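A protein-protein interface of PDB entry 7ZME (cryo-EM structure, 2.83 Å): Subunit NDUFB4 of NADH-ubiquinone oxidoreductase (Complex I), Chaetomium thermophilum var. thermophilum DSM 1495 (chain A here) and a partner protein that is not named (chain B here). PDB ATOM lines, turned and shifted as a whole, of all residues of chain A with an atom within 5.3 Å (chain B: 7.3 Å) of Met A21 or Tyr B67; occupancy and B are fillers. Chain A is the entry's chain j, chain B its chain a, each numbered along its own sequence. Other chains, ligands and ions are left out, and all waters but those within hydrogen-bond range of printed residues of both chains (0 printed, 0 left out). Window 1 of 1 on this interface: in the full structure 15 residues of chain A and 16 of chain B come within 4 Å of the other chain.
Of the printed residues of chain B, Ala A14 touches Val B97. Met A21 touches just these residues of chain B: Asn B64, Tyr B67 and Glu B99. Of the printed residues of chain A, Met B63 touches Arg A25 (3.7 Å). Tyr B67 touches just these residues of chain A: Arg A17 (3.6 Å), Leu A18 (3.8 Å) and Met A21 (3.7 Å). The nearest residue of chain B that does not touch Met A21 is Gly B65 (4.2 Å).
Among the printed residues, pairs that only touch across the chains: Leu A18 with His B98 (3.3 Å), Met A21 with Asn B64 (3.4 Å), Arg A25 with Asn B64 (3.6 Å), Arg A17 with Tyr B67 (3.6 Å), Met A21 with Tyr B67 (3.7 Å), Leu A18 with Val B97 (3.7 Å), Ala A14 with Val B97 (3.7 Å), Arg A25 with Met B63 (3.7 Å), Leu A18 with Glu B99 (3.7 Å), Leu A18 with Tyr B67 (3.8 Å) and Met A21 with Glu B99 (3.8 Å).
O of Asp B62 sits at hydrogen-bond distance from NH2 of Arg A25, at 2.8 Å. The guanidinium group of Arg A25 is in salt-bridge range of the side-chain carboxylate of Glu B99, 3.5 Å away.
The side-chain carboxylate (OD1) of Asp B60 lies within hydrogen-bond range of the backbone NH (N) of Met B63 (3.3 Å). The backbone NH of Gly B66 sits close to the side-chain amide oxygen of Asn B64, 3.3 Å away. A ring nitrogen (NE2) of His B98 sits at hydrogen-bond distance from the side-chain amide nitrogen (ND2) of Asn B69 (3.0 Å). The side-chain amide oxygen (OD1) of Asn B69 sits at hydrogen-bond distance from the backbone NH (N) of Glu B99, at 3.2 Å. ND1 of His B98 sits at hydrogen-bond distance from N of Asp B100 (2.9 Å). The backbone carbonyl oxygen of Arg A17 lies within hydrogen-bond range of the side-chain hydroxyl of Ser A20, 2.9 Å away.
Hydrophobic or aromatic side chains of chain A that line the printed part of chain B: Leu A18 and Met A21. Along chain A the printed residues that touch a printed residue of chain B span positions 14 to 25. Among the printed residues, Asp or Glu carboxylates within 4 Å of a Lys or Arg side-chain nitrogen of the other chain: Arg A25 with Glu B99 (3.5 Å).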
ATOM      1  N   ALA A  14      -4.311  20.035  -8.409  1.00  0.00           N
ATOM      2  CA  ALA A  14      -5.671  20.318  -7.957  1.00  0.00           C
ATOM      3  C   ALA A  14      -5.840  19.995  -6.479  1.00  0.00           C
ATOM      4  O   ALA A  14      -6.471  20.757  -5.738  1.00  0.00           O
ATOM      5  CB  ALA A  14      -6.675  19.532  -8.795  1.00  0.00           C
ATOM      6  N   ARG A  17      -4.084  22.561  -4.238  1.00  0.00           N
ATOM      7  CA  ARG A  17      -4.748  23.854  -4.175  1.00  0.00           C
ATOM      8  C   ARG A  17      -6.062  23.776  -3.419  1.00  0.00           C
ATOM      9  O   ARG A  17      -6.492  24.777  -2.837  1.00  0.00           O
ATOM     10  CB  ARG A  17      -4.968  24.412  -5.584  1.00  0.00           C
ATOM     11  CG  ARG A  17      -6.377  24.269  -6.130  1.00  0.00           C
ATOM     12  CD  ARG A  17      -6.464  24.784  -7.554  1.00  0.00           C
ATOM     13  NE  ARG A  17      -5.607  24.022  -8.456  1.00  0.00           N
ATOM     14  CZ  ARG A  17      -5.323  24.388  -9.702  1.00  0.00           C
ATOM     15  NH1 ARG A  17      -4.532  23.633 -10.452  1.00  0.00           N
ATOM     16  NH2 ARG A  17      -5.829  25.508 -10.198  1.00  0.00           N
ATOM     17  N   LEU A  18      -6.704  22.607  -3.407  1.00  0.00           N
ATOM     18  CA  LEU A  18      -7.835  22.395  -2.512  1.00  0.00           C
ATOM     19  C   LEU A  18      -7.397  22.462  -1.055  1.00  0.00           C
ATOM     20  O   LEU A  18      -8.066  23.089  -0.226  1.00  0.00           O
ATOM     21  CB  LEU A  18      -8.493  21.050  -2.813  1.00  0.00           C
ATOM     22  CG  LEU A  18      -9.759  20.706  -2.026  1.00  0.00           C
ATOM     23  CD1 LEU A  18     -10.755  21.841  -2.083  1.00  0.00           C
ATOM     24  CD2 LEU A  18     -10.376  19.433  -2.556  1.00  0.00           C
ATOM     25  N   GLY A  19      -6.271  21.828  -0.728  1.00  0.00           N
ATOM     26  CA  GLY A  19      -5.771  21.875   0.635  1.00  0.00           C
ATOM     27  C   GLY A  19      -5.355  23.269   1.060  1.00  0.00           C
ATOM     28  O   GLY A  19      -5.527  23.650   2.221  1.00  0.00           O
ATOM     29  N   SER A  20      -4.795  24.049   0.133  1.00  0.00           N
ATOM     30  CA  SER A  20      -4.436  25.427   0.449  1.00  0.00           C
ATOM     31  C   SER A  20      -5.676  26.286   0.647  1.00  0.00           C
ATOM     32  O   SER A  20      -5.698  27.157   1.522  1.00  0.00           O
ATOM     33  CB  SER A  20      -3.549  26.007  -0.650  1.00  0.00           C
ATOM     34  OG  SER A  20      -4.315  26.373  -1.782  1.00  0.00           O
ATOM     35  N   MET A  21      -6.716  26.059  -0.157  1.00  0.00           N
ATOM     36  CA  MET A  21      -7.965  26.792   0.020  1.00  0.00           C
ATOM     37  C   MET A  21      -8.614  26.461   1.355  1.00  0.00           C
ATOM     38  O   MET A  21      -9.085  27.357   2.064  1.00  0.00           O
ATOM     39  CB  MET A  21      -8.916  26.484  -1.141  1.00  0.00           C
ATOM     40  CG  MET A  21     -10.241  27.237  -1.108  1.00  0.00           C
ATOM     41  SD  MET A  21     -11.502  26.511  -0.039  1.00  0.00           S
ATOM     42  CE  MET A  21     -11.953  25.064  -0.984  1.00  0.00           C
ATOM     43  N   ILE A  22      -8.658  25.177   1.710  1.00  0.00           N
ATOM     44  CA  ILE A  22      -9.245  24.770   2.981  1.00  0.00           C
ATOM     45  C   ILE A  22      -8.441  25.341   4.140  1.00  0.00           C
ATOM     46  O   ILE A  22      -9.001  25.780   5.150  1.00  0.00           O
ATOM     47  CB  ILE A  22      -9.338  23.235   3.047  1.00  0.00           C
ATOM     48  CG1 ILE A  22     -10.401  22.729   2.072  1.00  0.00           C
ATOM     49  CG2 ILE A  22      -9.651  22.768   4.458  1.00  0.00           C
ATOM     50  CD1 ILE A  22     -10.294  21.255   1.769  1.00  0.00           C
ATOM     51  N   SER A  23      -7.113  25.357   4.005  1.00  0.00           N
ATOM     52  CA  SER A  23      -6.259  25.918   5.045  1.00  0.00           C
ATOM     53  C   SER A  23      -6.479  27.414   5.207  1.00  0.00           C
ATOM     54  O   SER A  23      -6.436  27.937   6.325  1.00  0.00           O
ATOM     55  CB  SER A  23      -4.793  25.632   4.729  1.00  0.00           C
ATOM     56  OG  SER A  23      -3.946  26.197   5.712  1.00  0.00           O
ATOM     57  N   ASN A  24      -6.700  28.122   4.103  1.00  0.00           N
ATOM     58  CA  ASN A  24      -6.793  29.574   4.100  1.00  0.00           C
ATOM     59  C   ASN A  24      -8.228  30.075   4.161  1.00  0.00           C
ATOM     60  O   ASN A  24      -8.455  31.283   4.058  1.00  0.00           O
ATOM     61  CB  ASN A  24      -6.108  30.135   2.854  1.00  0.00           C
ATOM     62  CG  ASN A  24      -4.608  30.000   2.906  1.00  0.00           C
ATOM     63  OD1 ASN A  24      -3.966  30.457   3.848  1.00  0.00           O
ATOM     64  ND2 ASN A  24      -4.035  29.391   1.883  1.00  0.00           N
ATOM     65  N   ARG A  25      -9.196  29.176   4.341  1.00  0.00           N
ATOM     66  CA  ARG A  25     -10.603  29.530   4.179  1.00  0.00           C
ATOM     67  C   ARG A  25     -11.065  30.565   5.199  1.00  0.00           C
ATOM     68  O   ARG A  25     -12.003  31.323   4.927  1.00  0.00           O
ATOM     69  CB  ARG A  25     -11.463  28.271   4.283  1.00  0.00           C
ATOM     70  CG  ARG A  25     -12.901  28.487   3.897  1.00  0.00           C
ATOM     71  CD  ARG A  25     -13.733  27.232   4.048  1.00  0.00           C
ATOM     72  NE  ARG A  25     -15.137  27.523   3.789  1.00  0.00           N
ATOM     73  CZ  ARG A  25     -15.713  27.416   2.598  1.00  0.00           C
ATOM     74  NH1 ARG A  25     -15.008  27.001   1.558  1.00  0.00           N
ATOM     75  NH2 ARG A  25     -16.995  27.712   2.449  1.00  0.00           N
ATOM     76  N   LEU B  55     -13.123  40.319   0.041  1.00  0.00           N
ATOM     77  CA  LEU B  55     -13.853  40.027  -1.185  1.00  0.00           C
ATOM     78  C   LEU B  55     -15.352  40.248  -1.006  1.00  0.00           C
ATOM     79  O   LEU B  55     -15.908  40.073   0.082  1.00  0.00           O
ATOM     80  CB  LEU B  55     -13.598  38.588  -1.628  1.00  0.00           C
ATOM     81  CG  LEU B  55     -12.136  38.173  -1.783  1.00  0.00           C
ATOM     82  CD1 LEU B  55     -12.039  36.721  -2.220  1.00  0.00           C
ATOM     83  CD2 LEU B  55     -11.418  39.087  -2.767  1.00  0.00           C
ATOM     84  N   GLU B  59     -17.793  38.100  -6.332  1.00  0.00           N
ATOM     85  CA  GLU B  59     -16.633  37.309  -6.715  1.00  0.00           C
ATOM     86  C   GLU B  59     -16.375  36.135  -5.782  1.00  0.00           C
ATOM     87  O   GLU B  59     -15.732  35.165  -6.197  1.00  0.00           O
ATOM     88  CB  GLU B  59     -15.383  38.194  -6.768  1.00  0.00           C
ATOM     89  CG  GLU B  59     -14.995  38.800  -5.429  1.00  0.00           C
ATOM     90  CD  GLU B  59     -14.110  40.022  -5.576  1.00  0.00           C
ATOM     91  OE1 GLU B  59     -14.156  40.901  -4.689  1.00  0.00           O
ATOM     92  OE2 GLU B  59     -13.369  40.105  -6.577  1.00  0.00           O
ATOM     93  N   ASP B  60     -16.858  36.195  -4.544  1.00  0.00           N
ATOM     94  CA  ASP B  60     -16.598  35.171  -3.534  1.00  0.00           C
ATOM     95  C   ASP B  60     -17.903  34.775  -2.855  1.00  0.00           C
ATOM     96  O   ASP B  60     -18.151  35.134  -1.699  1.00  0.00           O
ATOM     97  CB  ASP B  60     -15.580  35.677  -2.513  1.00  0.00           C
ATOM     98  CG  ASP B  60     -15.077  34.585  -1.601  1.00  0.00           C
ATOM     99  OD1 ASP B  60     -15.263  33.396  -1.936  1.00  0.00           O
ATOM    100  OD2 ASP B  60     -14.497  34.918  -0.547  1.00  0.00           O
ATOM    101  N   PRO B  61     -18.759  34.025  -3.546  1.00  0.00           N
ATOM    102  CA  PRO B  61     -20.052  33.659  -2.952  1.00  0.00           C
ATOM    103  C   PRO B  61     -19.953  32.505  -1.967  1.00  0.00           C
ATOM    104  O   PRO B  61     -20.734  32.429  -1.013  1.00  0.00           O
ATOM    105  CB  PRO B  61     -20.899  33.286  -4.172  1.00  0.00           C
ATOM    106  CG  PRO B  61     -19.910  32.786  -5.171  1.00  0.00           C
ATOM    107  CD  PRO B  61     -18.607  33.504  -4.916  1.00  0.00           C
ATOM    108  N   ASP B  62     -18.996  31.602  -2.182  1.00  0.00           N
ATOM    109  CA  ASP B  62     -18.830  30.438  -1.321  1.00  0.00           C
ATOM    110  C   ASP B  62     -17.963  30.711  -0.101  1.00  0.00           C
ATOM    111  O   ASP B  62     -17.763  29.799   0.707  1.00  0.00           O
ATOM    112  CB  ASP B  62     -18.235  29.279  -2.120  1.00  0.00           C
ATOM    113  CG  ASP B  62     -19.198  28.725  -3.151  1.00  0.00           C
ATOM    114  OD1 ASP B  62     -20.424  28.800  -2.924  1.00  0.00           O
ATOM    115  OD2 ASP B  62     -18.728  28.211  -4.188  1.00  0.00           O
ATOM    116  N   MET B  63     -17.442  31.930   0.045  1.00  0.00           N
ATOM    117  CA  MET B  63     -16.573  32.362   1.137  1.00  0.00           C
ATOM    118  C   MET B  63     -15.261  31.597   1.200  1.00  0.00           C
ATOM    119  O   MET B  63     -14.583  31.639   2.230  1.00  0.00           O
ATOM    120  CB  MET B  63     -17.263  32.278   2.500  1.00  0.00           C
ATOM    121  CG  MET B  63     -18.398  33.256   2.659  1.00  0.00           C
ATOM    122  SD  MET B  63     -19.190  33.133   4.258  1.00  0.00           S
ATOM    123  CE  MET B  63     -20.489  34.328   4.034  1.00  0.00           C
ATOM    124  N   ASN B  64     -14.889  30.888   0.143  1.00  0.00           N
ATOM    125  CA  ASN B  64     -13.532  30.391   0.005  1.00  0.00           C
ATOM    126  C   ASN B  64     -12.666  31.519  -0.555  1.00  0.00           C
ATOM    127  O   ASN B  64     -13.066  32.682  -0.572  1.00  0.00           O
ATOM    128  CB  ASN B  64     -13.509  29.133  -0.857  1.00  0.00           C
ATOM    129  CG  ASN B  64     -14.448  29.205  -2.036  1.00  0.00           C
ATOM    130  OD1 ASN B  64     -14.466  30.184  -2.777  1.00  0.00           O
ATOM    131  ND2 ASN B  64     -15.220  28.149  -2.232  1.00  0.00           N
ATOM    132  N   GLY B  65     -11.467  31.209  -1.016  1.00  0.00           N
ATOM    133  CA  GLY B  65     -10.627  32.269  -1.536  1.00  0.00           C
ATOM    134  C   GLY B  65     -11.021  32.743  -2.919  1.00  0.00           C
ATOM    135  O   GLY B  65     -10.197  33.304  -3.646  1.00  0.00           O
ATOM    136  N   GLY B  66     -12.276  32.533  -3.291  1.00  0.00           N
ATOM    137  CA  GLY B  66     -12.671  32.671  -4.676  1.00  0.00           C
ATOM    138  C   GLY B  66     -12.253  31.436  -5.444  1.00  0.00           C
ATOM    139  O   GLY B  66     -11.537  31.522  -6.444  1.00  0.00           O
ATOM    140  N   TYR B  67     -12.697  30.277  -4.972  1.00  0.00           N
ATOM    141  CA  TYR B  67     -12.263  28.995  -5.505  1.00  0.00           C
ATOM    142  C   TYR B  67     -13.211  28.539  -6.607  1.00  0.00           C
ATOM    143  O   TYR B  67     -14.423  28.452  -6.393  1.00  0.00           O
ATOM    144  CB  TYR B  67     -12.202  27.958  -4.381  1.00  0.00           C
ATOM    145  CG  TYR B  67     -11.579  26.642  -4.762  1.00  0.00           C
ATOM    146  CD1 TYR B  67     -10.210  26.453  -4.676  1.00  0.00           C
ATOM    147  CD2 TYR B  67     -12.362  25.580  -5.192  1.00  0.00           C
ATOM    148  CE1 TYR B  67      -9.633  25.247  -5.018  1.00  0.00           C
ATOM    149  CE2 TYR B  67     -11.797  24.372  -5.537  1.00  0.00           C
ATOM    150  CZ  TYR B  67     -10.430  24.211  -5.447  1.00  0.00           C
ATOM    151  OH  TYR B  67      -9.853  23.010  -5.788  1.00  0.00           O
ATOM    152  N   ILE B  68     -12.658  28.251  -7.779  1.00  0.00           N
ATOM    153  CA  ILE B  68     -13.459  27.793  -8.908  1.00  0.00           C
ATOM    154  C   ILE B  68     -13.850  26.344  -8.652  1.00  0.00           C
ATOM    155  O   ILE B  68     -12.989  25.489  -8.423  1.00  0.00           O
ATOM    156  CB  ILE B  68     -12.697  27.941 -10.231  1.00  0.00           C
ATOM    157  CG1 ILE B  68     -12.404  29.414 -10.508  1.00  0.00           C
ATOM    158  CG2 ILE B  68     -13.496  27.335 -11.375  1.00  0.00           C
ATOM    159  CD1 ILE B  68     -13.643  30.283 -10.541  1.00  0.00           C
ATOM    160  N   ASN B  69     -15.146  26.064  -8.701  1.00  0.00           N
ATOM    161  CA  ASN B  69     -15.677  24.811  -8.192  1.00  0.00           C
ATOM    162  C   ASN B  69     -16.407  24.069  -9.304  1.00  0.00           C
ATOM    163  O   ASN B  69     -17.352  24.622  -9.892  1.00  0.00           O
ATOM    164  CB  ASN B  69     -16.617  25.087  -7.022  1.00  0.00           C
ATOM    165  CG  ASN B  69     -16.589  23.997  -5.988  1.00  0.00           C
ATOM    166  OD1 ASN B  69     -15.867  23.019  -6.132  1.00  0.00           O
ATOM    167  ND2 ASN B  69     -17.360  24.167  -4.925  1.00  0.00           N
ATOM    168  N   PRO B  70     -16.017  22.842  -9.634  1.00  0.00           N
ATOM    169  CA  PRO B  70     -16.739  22.078 -10.652  1.00  0.00           C
ATOM    170  C   PRO B  70     -18.119  21.692 -10.152  1.00  0.00           C
ATOM    171  O   PRO B  70     -18.404  21.819  -8.952  1.00  0.00           O
ATOM    172  CB  PRO B  70     -15.855  20.840 -10.867  1.00  0.00           C
ATOM    173  CG  PRO B  70     -15.005  20.749  -9.675  1.00  0.00           C
ATOM    174  CD  PRO B  70     -14.840  22.124  -9.123  1.00  0.00           C
ATOM    175  N   PRO B  96      -9.640  19.073 -12.042  1.00  0.00           N
ATOM    176  CA  PRO B  96     -10.072  19.917 -10.924  1.00  0.00           C
ATOM    177  C   PRO B  96     -11.016  19.165 -10.000  1.00  0.00           C
ATOM    178  O   PRO B  96     -11.710  18.232 -10.406  1.00  0.00           O
ATOM    179  CB  PRO B  96     -10.778  21.093 -11.613  1.00  0.00           C
ATOM    180  CG  PRO B  96     -11.058  20.624 -13.002  1.00  0.00           C
ATOM    181  CD  PRO B  96      -9.966  19.671 -13.344  1.00  0.00           C
ATOM    182  N   VAL B  97     -11.024  19.578  -8.737  1.00  0.00           N
ATOM    183  CA  VAL B  97     -11.772  18.893  -7.693  1.00  0.00           C
ATOM    184  C   VAL B  97     -12.743  19.875  -7.052  1.00  0.00           C
ATOM    185  O   VAL B  97     -12.571  21.093  -7.116  1.00  0.00           O
ATOM    186  CB  VAL B  97     -10.839  18.280  -6.628  1.00  0.00           C
ATOM    187  CG1 VAL B  97     -10.135  17.057  -7.175  1.00  0.00           C
ATOM    188  CG2 VAL B  97      -9.831  19.304  -6.168  1.00  0.00           C
ATOM    189  N   HIS B  98     -13.774  19.323  -6.428  1.00  0.00           N
ATOM    190  CA  HIS B  98     -14.743  20.106  -5.680  1.00  0.00           C
ATOM    191  C   HIS B  98     -14.260  20.310  -4.249  1.00  0.00           C
ATOM    192  O   HIS B  98     -13.423  19.564  -3.741  1.00  0.00           O
ATOM    193  CB  HIS B  98     -16.106  19.414  -5.684  1.00  0.00           C
ATOM    194  CG  HIS B  98     -17.245  20.305  -5.307  1.00  0.00           C
ATOM    195  ND1 HIS B  98     -17.601  20.545  -3.998  1.00  0.00           N
ATOM    196  CD2 HIS B  98     -18.119  21.005  -6.066  1.00  0.00           C
ATOM    197  CE1 HIS B  98     -18.636  21.363  -3.966  1.00  0.00           C
ATOM    198  NE2 HIS B  98     -18.970  21.656  -5.208  1.00  0.00           N
ATOM    199  N   GLU B  99     -14.799  21.339  -3.595  1.00  0.00           N
ATOM    200  CA  GLU B  99     -14.489  21.526  -2.184  1.00  0.00           C
ATOM    201  C   GLU B  99     -15.043  20.407  -1.315  1.00  0.00           C
ATOM    202  O   GLU B  99     -14.640  20.289  -0.154  1.00  0.00           O
ATOM    203  CB  GLU B  99     -15.004  22.881  -1.695  1.00  0.00           C
ATOM    204  CG  GLU B  99     -16.490  22.947  -1.438  1.00  0.00           C
ATOM    205  CD  GLU B  99     -17.021  24.365  -1.516  1.00  0.00           C
ATOM    206  OE1 GLU B  99     -17.411  24.800  -2.620  1.00  0.00           O
ATOM    207  OE2 GLU B  99     -17.040  25.051  -0.473  1.00  0.00           O
ATOM    208  N   ASP B 100     -15.948  19.584  -1.849  1.00  0.00           N
ATOM    209  CA  ASP B 100     -16.402  18.357  -1.209  1.00  0.00           C
ATOM    210  C   ASP B 100     -15.774  17.120  -1.843  1.00  0.00           C
ATOM    211  O   ASP B 100     -16.425  16.076  -1.940  1.00  0.00           O
ATOM    212  CB  ASP B 100     -17.925  18.261  -1.259  1.00  0.00           C
ATOM    213  CG  ASP B 100     -18.601  19.329  -0.431  1.00  0.00           C
ATOM    214  OD1 ASP B 100     -17.887  20.157   0.166  1.00  0.00           O
ATOM    215  OD2 ASP B 100     -19.847  19.342  -0.376  1.00  0.00           O
